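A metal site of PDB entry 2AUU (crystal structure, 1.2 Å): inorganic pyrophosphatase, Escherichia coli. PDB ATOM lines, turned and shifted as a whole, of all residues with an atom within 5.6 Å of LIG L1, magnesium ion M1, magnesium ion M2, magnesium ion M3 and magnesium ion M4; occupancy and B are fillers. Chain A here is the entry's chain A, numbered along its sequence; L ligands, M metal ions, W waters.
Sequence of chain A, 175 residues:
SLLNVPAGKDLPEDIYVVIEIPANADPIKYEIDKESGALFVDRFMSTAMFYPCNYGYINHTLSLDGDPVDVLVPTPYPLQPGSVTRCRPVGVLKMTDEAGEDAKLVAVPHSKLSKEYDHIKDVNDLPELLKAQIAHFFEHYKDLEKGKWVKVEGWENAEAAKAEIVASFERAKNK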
ATOM      1  N   GLU A  20      16.607  -4.440  18.911  1.00  0.00           N
ATOM      2  CA  GLU A  20      16.837  -3.862  20.235  1.00  0.00           C
ATOM      3  C   GLU A  20      16.471  -4.772  21.397  1.00  0.00           C
ATOM      4  O   GLU A  20      17.123  -4.756  22.409  1.00  0.00           O
ATOM      5  CB  GLU A  20      16.032  -2.571  20.335  1.00  0.00           C
ATOM      6  CG  GLU A  20      16.609  -1.501  19.397  1.00  0.00           C
ATOM      7  CD  GLU A  20      15.651  -0.304  19.302  1.00  0.00           C
ATOM      8  OE1 GLU A  20      14.456  -0.544  19.152  1.00  0.00           O
ATOM      9  OE2 GLU A  20      16.172   0.861  19.389  1.00  0.00           O
ATOM     10  N   LYS A  29      13.664  -2.592  28.447  1.00  0.00           N
ATOM     11  CA  LYS A  29      13.350  -1.939  27.171  1.00  0.00           C
ATOM     12  C   LYS A  29      14.567  -1.194  26.697  1.00  0.00           C
ATOM     13  O   LYS A  29      14.826  -0.086  27.098  1.00  0.00           O
ATOM     14  CB  LYS A  29      12.152  -1.037  27.368  1.00  0.00           C
ATOM     15  CG  LYS A  29      11.392  -0.741  26.172  1.00  0.00           C
ATOM     16  CD  LYS A  29      11.983  -0.055  25.024  1.00  0.00           C
ATOM     17  CE  LYS A  29      10.912   0.061  23.909  1.00  0.00           C
ATOM     18  NZ  LYS A  29      11.415   0.825  22.723  1.00  0.00           N
ATOM     19  N   GLU A  31      16.875   0.741  23.794  1.00  0.00           N
ATOM     20  CA  GLU A  31      16.736   1.515  22.592  1.00  0.00           C
ATOM     21  C   GLU A  31      18.112   1.957  22.136  1.00  0.00           C
ATOM     22  O   GLU A  31      18.877   2.433  22.960  1.00  0.00           O
ATOM     23  CB  GLU A  31      15.831   2.743  22.793  1.00  0.00           C
ATOM     24  CG  GLU A  31      14.381   2.391  23.099  1.00  0.00           C
ATOM     25  CD  GLU A  31      13.451   3.589  23.131  1.00  0.00           C
ATOM     26  OE1 GLU A  31      13.881   4.745  22.985  1.00  0.00           O
ATOM     27  OE2 GLU A  31      12.195   3.419  23.318  1.00  0.00           O
ATOM     28  N   ASP A  42      16.199   2.141  28.070  1.00  0.00           N
ATOM     29  CA  ASP A  42      15.229   3.195  28.089  1.00  0.00           C
ATOM     30  C   ASP A  42      14.460   3.133  29.388  1.00  0.00           C
ATOM     31  O   ASP A  42      14.243   4.159  30.059  1.00  0.00           O
ATOM     32  CB  ASP A  42      14.321   3.145  26.842  1.00  0.00           C
ATOM     33  CG  ASP A  42      13.371   4.314  26.853  1.00  0.00           C
ATOM     34  OD1 ASP A  42      13.786   5.462  26.642  1.00  0.00           O
ATOM     35  OD2 ASP A  42      12.205   4.102  27.115  1.00  0.00           O
ATOM     36  N   ARG A  43      14.003   1.934  29.748  1.00  0.00           N
ATOM     37  CA  ARG A  43      13.367   1.738  31.038  1.00  0.00           C
ATOM     38  C   ARG A  43      13.279   0.241  31.344  1.00  0.00           C
ATOM     39  O   ARG A  43      13.542  -0.604  30.484  1.00  0.00           O
ATOM     40  CB  ARG A  43      12.018   2.358  31.036  1.00  0.00           C
ATOM     41  CG  ARG A  43      11.060   1.617  30.105  1.00  0.00           C
ATOM     42  CD  ARG A  43       9.890   2.509  29.785  1.00  0.00           C
ATOM     43  NE  ARG A  43       8.893   1.868  28.934  1.00  0.00           N
ATOM     44  CZ  ARG A  43       8.833   1.928  27.600  1.00  0.00           C
ATOM     45  NH1 ARG A  43       9.733   2.615  26.863  1.00  0.00           N
ATOM     46  NH2 ARG A  43       7.834   1.278  26.955  1.00  0.00           N
ATOM     47  N   TYR A  51       7.964  -9.157  24.862  1.00  0.00           N
ATOM     48  CA  TYR A  51       7.679  -8.936  23.459  1.00  0.00           C
ATOM     49  C   TYR A  51       7.445 -10.283  22.757  1.00  0.00           C
ATOM     50  O   TYR A  51       8.307 -11.189  22.888  1.00  0.00           O
ATOM     51  CB  TYR A  51       8.795  -8.214  22.719  1.00  0.00           C
ATOM     52  CG  TYR A  51       8.805  -6.741  23.036  1.00  0.00           C
ATOM     53  CD1 TYR A  51       9.298  -6.202  24.206  1.00  0.00           C
ATOM     54  CD2 TYR A  51       8.299  -5.794  22.125  1.00  0.00           C
ATOM     55  CE1 TYR A  51       9.308  -4.874  24.523  1.00  0.00           C
ATOM     56  CE2 TYR A  51       8.298  -4.461  22.421  1.00  0.00           C
ATOM     57  CZ  TYR A  51       8.796  -3.985  23.618  1.00  0.00           C
ATOM     58  OH  TYR A  51       8.824  -2.682  23.934  1.00  0.00           O
ATOM     59  N   TYR A  55      12.174  -7.283  18.547  1.00  0.00           N
ATOM     60  CA  TYR A  55      11.679  -5.942  18.326  1.00  0.00           C
ATOM     61  C   TYR A  55      12.841  -4.993  18.013  1.00  0.00           C
ATOM     62  O   TYR A  55      13.856  -5.020  18.690  1.00  0.00           O
ATOM     63  CB  TYR A  55      10.978  -5.458  19.567  1.00  0.00           C
ATOM     64  CG  TYR A  55      10.384  -4.086  19.490  1.00  0.00           C
ATOM     65  CD1 TYR A  55       9.173  -3.898  18.847  1.00  0.00           C
ATOM     66  CD2 TYR A  55      10.992  -2.987  20.058  1.00  0.00           C
ATOM     67  CE1 TYR A  55       8.613  -2.662  18.774  1.00  0.00           C
ATOM     68  CE2 TYR A  55      10.441  -1.735  19.974  1.00  0.00           C
ATOM     69  CZ  TYR A  55       9.247  -1.572  19.330  1.00  0.00           C
ATOM     70  OH  TYR A  55       8.590  -0.363  19.210  1.00  0.00           O
ATOM     71  N   GLY A  56      12.668  -4.158  16.977  1.00  0.00           N
ATOM     72  CA  GLY A  56      13.682  -3.186  16.652  1.00  0.00           C
ATOM     73  C   GLY A  56      13.153  -2.153  15.690  1.00  0.00           C
ATOM     74  O   GLY A  56      12.011  -1.746  15.766  1.00  0.00           O
ATOM     75  N   TYR A  57      14.017  -1.747  14.776  1.00  0.00           N
ATOM     76  CA  TYR A  57      13.697  -0.641  13.843  1.00  0.00           C
ATOM     77  C   TYR A  57      14.425  -0.774  12.534  1.00  0.00           C
ATOM     78  O   TYR A  57      15.370  -1.526  12.389  1.00  0.00           O
ATOM     79  CB  TYR A  57      14.020   0.696  14.567  1.00  0.00           C
ATOM     80  CG  TYR A  57      15.467   0.893  14.789  1.00  0.00           C
ATOM     81  CD1 TYR A  57      16.065   0.387  15.909  1.00  0.00           C
ATOM     82  CD2 TYR A  57      16.312   1.565  13.902  1.00  0.00           C
ATOM     83  CE1 TYR A  57      17.415   0.573  16.111  1.00  0.00           C
ATOM     84  CE2 TYR A  57      17.691   1.756  14.096  1.00  0.00           C
ATOM     85  CZ  TYR A  57      18.229   1.213  15.228  1.00  0.00           C
ATOM     86  OH  TYR A  57      19.555   1.356  15.525  1.00  0.00           O
ATOM     87  N   SER A  63       9.601   7.813  12.041  1.00  0.00           N
ATOM     88  CA  SER A  63       8.197   7.774  12.381  1.00  0.00           C
ATOM     89  C   SER A  63       7.722   9.084  13.019  1.00  0.00           C
ATOM     90  O   SER A  63       8.557   9.940  13.109  1.00  0.00           O
ATOM     91  CB  SER A  63       7.878   6.606  13.372  1.00  0.00           C
ATOM     92  OG  SER A  63       7.849   5.521  12.501  1.00  0.00           O
ATOM     93  N   ASP A  65       6.734   9.460  16.127  1.00  0.00           N
ATOM     94  CA  ASP A  65       7.056   9.406  17.536  1.00  0.00           C
ATOM     95  C   ASP A  65       8.512   9.875  17.776  1.00  0.00           C
ATOM     96  O   ASP A  65       9.011   9.789  18.906  1.00  0.00           O
ATOM     97  CB  ASP A  65       6.830   7.992  18.132  1.00  0.00           C
ATOM     98  CG  ASP A  65       7.834   6.929  17.743  1.00  0.00           C
ATOM     99  OD1 ASP A  65       7.977   5.891  18.446  1.00  0.00           O
ATOM    100  OD2 ASP A  65       8.449   7.200  16.692  1.00  0.00           O
ATOM    101  N   ASP A  67      11.158   8.594  16.359  1.00  0.00           N
ATOM    102  CA  ASP A  67      12.054   7.483  16.391  1.00  0.00           C
ATOM    103  C   ASP A  67      12.022   6.830  15.002  1.00  0.00           C
ATOM    104  O   ASP A  67      11.022   7.047  14.386  1.00  0.00           O
ATOM    105  CB  ASP A  67      11.629   6.445  17.428  1.00  0.00           C
ATOM    106  CG  ASP A  67      11.643   6.784  18.885  1.00  0.00           C
ATOM    107  OD1 ASP A  67      12.199   7.868  19.183  1.00  0.00           O
ATOM    108  OD2 ASP A  67      11.143   6.038  19.777  1.00  0.00           O
ATOM    109  N   PRO A  68      12.986   6.038  14.550  1.00  0.00           N
ATOM    110  CA  PRO A  68      12.821   5.139  13.378  1.00  0.00           C
ATOM    111  C   PRO A  68      11.633   4.192  13.469  1.00  0.00           C
ATOM    112  O   PRO A  68      11.215   3.842  14.592  1.00  0.00           O
ATOM    113  CB  PRO A  68      14.087   4.302  13.442  1.00  0.00           C
ATOM    114  CG  PRO A  68      15.125   5.190  14.101  1.00  0.00           C
ATOM    115  CD  PRO A  68      14.365   5.939  15.130  1.00  0.00           C
ATOM    116  N   ASP A  70       9.295   1.137  13.729  1.00  0.00           N
ATOM    117  CA  ASP A  70       9.409  -0.034  14.587  1.00  0.00           C
ATOM    118  C   ASP A  70       8.932  -1.272  13.920  1.00  0.00           C
ATOM    119  O   ASP A  70       7.923  -1.289  13.162  1.00  0.00           O
ATOM    120  CB  ASP A  70       8.556   0.226  15.819  1.00  0.00           C
ATOM    121  CG  ASP A  70       8.983   1.387  16.707  1.00  0.00           C
ATOM    122  OD1 ASP A  70      10.210   1.500  16.893  1.00  0.00           O
ATOM    123  OD2 ASP A  70       8.118   2.083  17.282  1.00  0.00           O
ATOM    124  N   MET A  95      -1.143   1.831  15.416  1.00  0.00           N
ATOM    125  CA  MET A  95      -1.359   2.325  16.768  1.00  0.00           C
ATOM    126  C   MET A  95      -0.675   3.701  16.996  1.00  0.00           C
ATOM    127  O   MET A  95       0.296   4.055  16.278  1.00  0.00           O
ATOM    128  CB  MET A  95      -0.892   1.320  17.821  1.00  0.00           C
ATOM    129  CG  MET A  95       0.502   0.814  17.490  1.00  0.00           C
ATOM    130  SD  MET A  95       1.436   0.463  18.997  1.00  0.00           S
ATOM    131  CE  MET A  95       1.638   2.135  19.621  1.00  0.00           C
ATOM    132  N   ASP A  97       0.990   6.319  20.333  1.00  0.00           N
ATOM    133  CA  ASP A  97       1.251   6.271  21.798  1.00  0.00           C
ATOM    134  C   ASP A  97       1.556   7.708  22.194  1.00  0.00           C
ATOM    135  O   ASP A  97       1.364   8.632  21.398  1.00  0.00           O
ATOM    136  CB  ASP A  97       2.258   5.246  22.219  1.00  0.00           C
ATOM    137  CG  ASP A  97       3.744   5.405  21.911  1.00  0.00           C
ATOM    138  OD1 ASP A  97       4.053   6.548  21.498  1.00  0.00           O
ATOM    139  OD2 ASP A  97       4.557   4.485  22.039  1.00  0.00           O
ATOM    140  N   GLU A  98       1.996   7.852  23.461  1.00  0.00           N
ATOM    141  CA  GLU A  98       2.195   9.191  24.000  1.00  0.00           C
ATOM    142  C   GLU A  98       3.168  10.026  23.190  1.00  0.00           C
ATOM    143  O   GLU A  98       3.053  11.242  23.268  1.00  0.00           O
ATOM    144  CB  GLU A  98       2.695   9.063  25.430  1.00  0.00           C
ATOM    145  CG  GLU A  98       4.177   8.768  25.618  1.00  0.00           C
ATOM    146  CD  GLU A  98       4.511   7.275  25.448  1.00  0.00           C
ATOM    147  OE1 GLU A  98       3.554   6.425  25.582  1.00  0.00           O
ATOM    148  OE2 GLU A  98       5.738   7.082  25.167  1.00  0.00           O
ATOM    149  N   ASP A 102       2.690   5.675  15.836  1.00  0.00           N
ATOM    150  CA  ASP A 102       3.757   4.711  16.077  1.00  0.00           C
ATOM    151  C   ASP A 102       3.449   3.326  15.597  1.00  0.00           C
ATOM    152  O   ASP A 102       3.431   2.412  16.428  1.00  0.00           O
ATOM    153  CB  ASP A 102       3.957   4.777  17.603  1.00  0.00           C
ATOM    154  CG  ASP A 102       5.293   4.250  18.018  1.00  0.00           C
ATOM    155  OD1 ASP A 102       6.316   4.093  17.272  1.00  0.00           O
ATOM    156  OD2 ASP A 102       5.280   3.954  19.272  1.00  0.00           O
ATOM    157  N   LYS A 104       3.466  -0.483  14.223  1.00  0.00           N
ATOM    158  CA  LYS A 104       4.284  -1.654  14.520  1.00  0.00           C
ATOM    159  C   LYS A 104       4.231  -2.625  13.295  1.00  0.00           C
ATOM    160  O   LYS A 104       3.286  -3.341  13.081  1.00  0.00           O
ATOM    161  CB  LYS A 104       3.869  -2.367  15.759  1.00  0.00           C
ATOM    162  CG  LYS A 104       3.880  -1.474  17.009  1.00  0.00           C
ATOM    163  CD  LYS A 104       5.272  -1.159  17.463  1.00  0.00           C
ATOM    164  CE  LYS A 104       5.272  -0.195  18.652  1.00  0.00           C
ATOM    165  NZ  LYS A 104       5.568   1.162  18.231  1.00  0.00           N
ATOM    166  N   TYR A 141       1.066  -3.247  27.636  1.00  0.00           N
ATOM    167  CA  TYR A 141       2.413  -3.178  28.201  1.00  0.00           C
ATOM    168  C   TYR A 141       2.705  -1.843  28.917  1.00  0.00           C
ATOM    169  O   TYR A 141       3.602  -1.845  29.751  1.00  0.00           O
ATOM    170  CB  TYR A 141       3.466  -3.476  27.166  1.00  0.00           C
ATOM    171  CG  TYR A 141       3.841  -2.383  26.189  1.00  0.00           C
ATOM    172  CD1 TYR A 141       2.859  -1.677  25.426  1.00  0.00           C
ATOM    173  CD2 TYR A 141       5.193  -2.056  26.021  1.00  0.00           C
ATOM    174  CE1 TYR A 141       3.293  -0.681  24.534  1.00  0.00           C
ATOM    175  CE2 TYR A 141       5.596  -1.077  25.159  1.00  0.00           C
ATOM    176  CZ  TYR A 141       4.641  -0.394  24.424  1.00  0.00           C
ATOM    177  OH  TYR A 141       5.001   0.631  23.512  1.00  0.00           O
ATOM    178  N   LYS A 142       1.991  -0.791  28.629  1.00  0.00           N
ATOM    179  CA  LYS A 142       2.165   0.491  29.261  1.00  0.00           C
ATOM    180  C   LYS A 142       1.163   0.761  30.360  1.00  0.00           C
ATOM    181  O   LYS A 142       1.088   1.920  30.790  1.00  0.00           O
ATOM    182  CB  LYS A 142       2.109   1.589  28.161  1.00  0.00           C
ATOM    183  CG  LYS A 142       3.468   1.651  27.375  1.00  0.00           C
ATOM    184  CD  LYS A 142       3.445   2.608  26.189  1.00  0.00           C
ATOM    185  CE  LYS A 142       4.830   3.127  25.819  1.00  0.00           C
ATOM    186  NZ  LYS A 142       4.834   3.907  24.588  1.00  0.00           N
ATOM    187  N   LYS A 148       2.522   7.114  29.818  1.00  0.00           N
ATOM    188  CA  LYS A 148       2.781   6.316  28.624  1.00  0.00           C
ATOM    189  C   LYS A 148       1.451   5.676  28.231  1.00  0.00           C
ATOM    190  O   LYS A 148       0.774   5.149  29.102  1.00  0.00           O
ATOM    191  CB  LYS A 148       3.751   5.187  28.773  1.00  0.00           C
ATOM    192  CG  LYS A 148       5.071   5.672  29.385  1.00  0.00           C
ATOM    193  CD  LYS A 148       6.099   6.239  28.494  1.00  0.00           C
ATOM    194  CE  LYS A 148       7.566   5.926  28.864  1.00  0.00           C
ATOM    195  NZ  LYS A 148       8.467   6.583  27.861  1.00  0.00           N
HETATM  196  P1  LIG L   1       8.074   2.547  23.364  1.00  0.00           P
HETATM  197  O1  LIG L   1       7.067   3.515  22.937  1.00  0.00           O
HETATM  198  O2  LIG L   1       7.603   1.350  24.119  1.00  0.00           O
HETATM  199  O3  LIG L   1       9.337   3.183  23.954  1.00  0.00           O
HETATM  200  O4  LIG L   1       8.749   1.834  21.973  1.00  0.00           O
HETATM  201  P2  LIG L   1       9.259   2.781  20.770  1.00  0.00           P
HETATM  202  O5  LIG L   1       8.074   3.353  20.030  1.00  0.00           O
HETATM  203  O6  LIG L   1      10.036   1.796  19.981  1.00  0.00           O
HETATM  204  O7  LIG L   1      10.076   3.835  21.491  1.00  0.00           O
HETATM  205  F1  LG2 L   2      10.225   3.987  18.438  1.00  0.00           F
HETATM  206 MG    MG M   1       8.216   4.009  18.144  1.00  0.00          MG
HETATM  207 MG    MG M   2      11.280   2.385  18.444  1.00  0.00          MG
HETATM  208 MG    MG M   3       6.202   3.799  21.146  1.00  0.00          MG
HETATM  209 MG    MG M   4      10.479   4.616  23.273  1.00  0.00          MG
HETATM  210  O   HOH W   1       7.654  -0.914  22.183  1.00  0.00           O
HETATM  211  O   HOH W   2      12.350   0.609  18.359  1.00  0.00           O
HETATM  212  O   HOH W   3       6.767   5.769  21.006  1.00  0.00           O
HETATM  213  O   HOH W   4       8.937   5.930  23.051  1.00  0.00           O
HETATM  214  O   HOH W   5      12.469   3.154  20.021  1.00  0.00           O
HETATM  215  O   HOH W   6       8.808   4.595  16.078  1.00  0.00           O
HETATM  216  O   HOH W   7      10.823   5.414  25.090  1.00  0.00           O
HETATM  217  O   HOH W   8       5.371   1.824  21.130  1.00  0.00           O
HETATM  218  O   HOH W   9      11.597   6.073  22.446  1.00  0.00           O
HETATM  219  O   HOH W  10      12.509   3.242  17.040  1.00  0.00           O
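Magnesium ion M2 is bound by F1 of LG2 L2 (1.9 Å).
Magnesium ion M2 is bound by water W10 (2.1 Å).
O6 of LIG L1 binds magnesium ion M2, 2.1 Å away.
Water W2 is bound to magnesium ion M2 (2.1 Å).
The side-chain carboxylate (OD1) of Asp 70 binds magnesium ion M2, 2.1 Å away.
Magnesium ion M2 is bound by water W5 (2.1 Å).
Magnesium ion M2 has six donor atoms within binding distance.
Magnesium ion M4 is bound by O3 of LIG L1, 2.0 Å away.
An oxygen (O7) of LIG L1 binds magnesium ion M4, 2.0 Å away.
Water W7 binds magnesium ion M4 (2.0 Å).
Magnesium ion M4 is bound by water W9, 2.0 Å away.
Water W4 binds magnesium ion M4, 2.0 Å away.
The side-chain carboxylate (OE2) of Glu 31 binds magnesium ion M4, at 2.1 Å.
Water W6 bridges the side-chain carboxylate of Asp 65 (2.7 Å) and the backbone carbonyl oxygen of Pro 68 (2.9 Å).
Water W8 lies within hydrogen-bond range of the side-chain hydroxyl of Tyr 141 (2.7 Å), the side-chain amino group of Lys 104 (3.0 Å) and an oxygen (O4) of LIG L1 (3.5 Å).
Water W9 bridges OE1 of Glu 31 and OD2 of Asp 67.
Water W7 bridges OD2 of Asp 42 (2.8 Å) and NH1 of Arg 43 (3.5 Å).
Water W1 lies within hydrogen-bond range of the side-chain hydroxyl of Tyr 51 (2.7 Å), an oxygen (O4) of LIG L1 (3.0 Å), the side-chain hydroxyl of Tyr 55 (3.2 Å) and the side-chain hydroxyl of Tyr 141 (3.3 Å).
The side-chain carboxylate (OD2) of Asp 70 lies close to the side-chain hydroxyl (OH) of Tyr 55.
The side-chain carboxylate (OE2) of Glu 31 sits close to the side-chain amino group (NZ) of Lys 29 (2.8 Å).
The backbone carbonyl oxygen (O) of Asp 102 sits at hydrogen-bond distance from the side-chain amino group (NZ) of Lys 104 (3.1 Å).
The backbone NH (N) of Glu 20 lies within hydrogen-bond range of the backbone carbonyl oxygen (O) of Tyr 55, at 2.8 Å.
The side-chain carboxylate (OD2) of Asp 65 sits at hydrogen-bond distance from the backbone NH (N) of Asp 67, at 3.1 Å.
NH1 of Arg 43 is in salt-bridge range of OD2 of Asp 42, 2.9 Å away.
NZ of Lys 104 sits close to OD2 of Asp 70, 2.9 Å away.
N of Lys 29 sits at hydrogen-bond distance from O of Arg 43, at 2.8 Å.
Merely in contact with magnesium ion M1: Asp 67 (3.9 Å) and Lys 104 (3.9 Å).
Of the 22 residues printed, 5 come within 4 Å of magnesium ion M1.
The nearest printed residue that does not touch magnesium ion M1 is Tyr 55 (4.5 Å).
Lys 29 touches magnesium ion M4.
OD2 of Asp 67 touches magnesium ion M4, 3.8 Å away.
Within 4 Å of magnesium ion M4: Lys 29, Glu 31 and Asp 67.
The nearest printed residue that does not touch magnesium ion M4 is Arg 43 (4.2 Å).
OH of Tyr 55 touches magnesium ion M2, at 3.9 Å.
Asp 67 touches magnesium ion M2 (OD2 to MG, 3.9 Å).
Within 4 Å of magnesium ion M2: Tyr 55, Asp 67 and Asp 70.
Along chain A the residues within 4 Å of magnesium ion M2 span positions 55 to 70.
Magnesium ion M1 is bound by OD1 of Asp 65 (1.9 Å), O5 of LIG L1 (2.0 Å), F1 of LG2 L2 (2.0 Å), OD1 of Asp 102 (2.1 Å), OD2 of Asp 70 (2.1 Å) and water W6 (2.2 Å).
Magnesium ion M1 has six donor atoms within binding distance.
NZ of Lys 104 touches magnesium ion M3, at 3.98 Å.
Lys 142 touches magnesium ion M3.
The nearest printed residue that does not touch magnesium ion M3 is Tyr 141 (4.1 Å).
NZ of Lys 29 sits at hydrogen-bond distance from O4 of LIG L1.
NH2 of Arg 43 is in salt-bridge range of O2 of LIG L1, at 2.8 Å.
An oxygen (O6) of LIG L1 sits close to the side-chain hydroxyl (OH) of Tyr 55 (2.7 Å).
The side-chain hydroxyl (OH) of Tyr 141 sits at hydrogen-bond distance from an oxygen (O2) of LIG L1.
The side-chain amino group (NZ) of Lys 104 lies close to an oxygen (O5) of LIG L1, 3.8 Å away.
NZ of Lys 142 lies within salt-bridge range of O2 of LIG L1 (3.8 Å).
An oxygen (O7) of LIG L1 sits close to the side-chain carboxylate (OD2) of Asp 67 (3.0 Å).
Of the 22 residues printed, 12 come within 4 Å of LIG L1.
The nearest printed residue that does not touch LIG L1 is Tyr 51 (4.2 Å).
Magnesium ion M3 is bound by the side-chain carboxylate (OD2) of Asp 97, an oxygen (O1) of LIG L1, water W3, the side-chain carboxylate (OD2) of Asp 102, water W8 and an oxygen (O5) of LIG L1.
Magnesium ion M3 has six donor atoms within binding distance.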
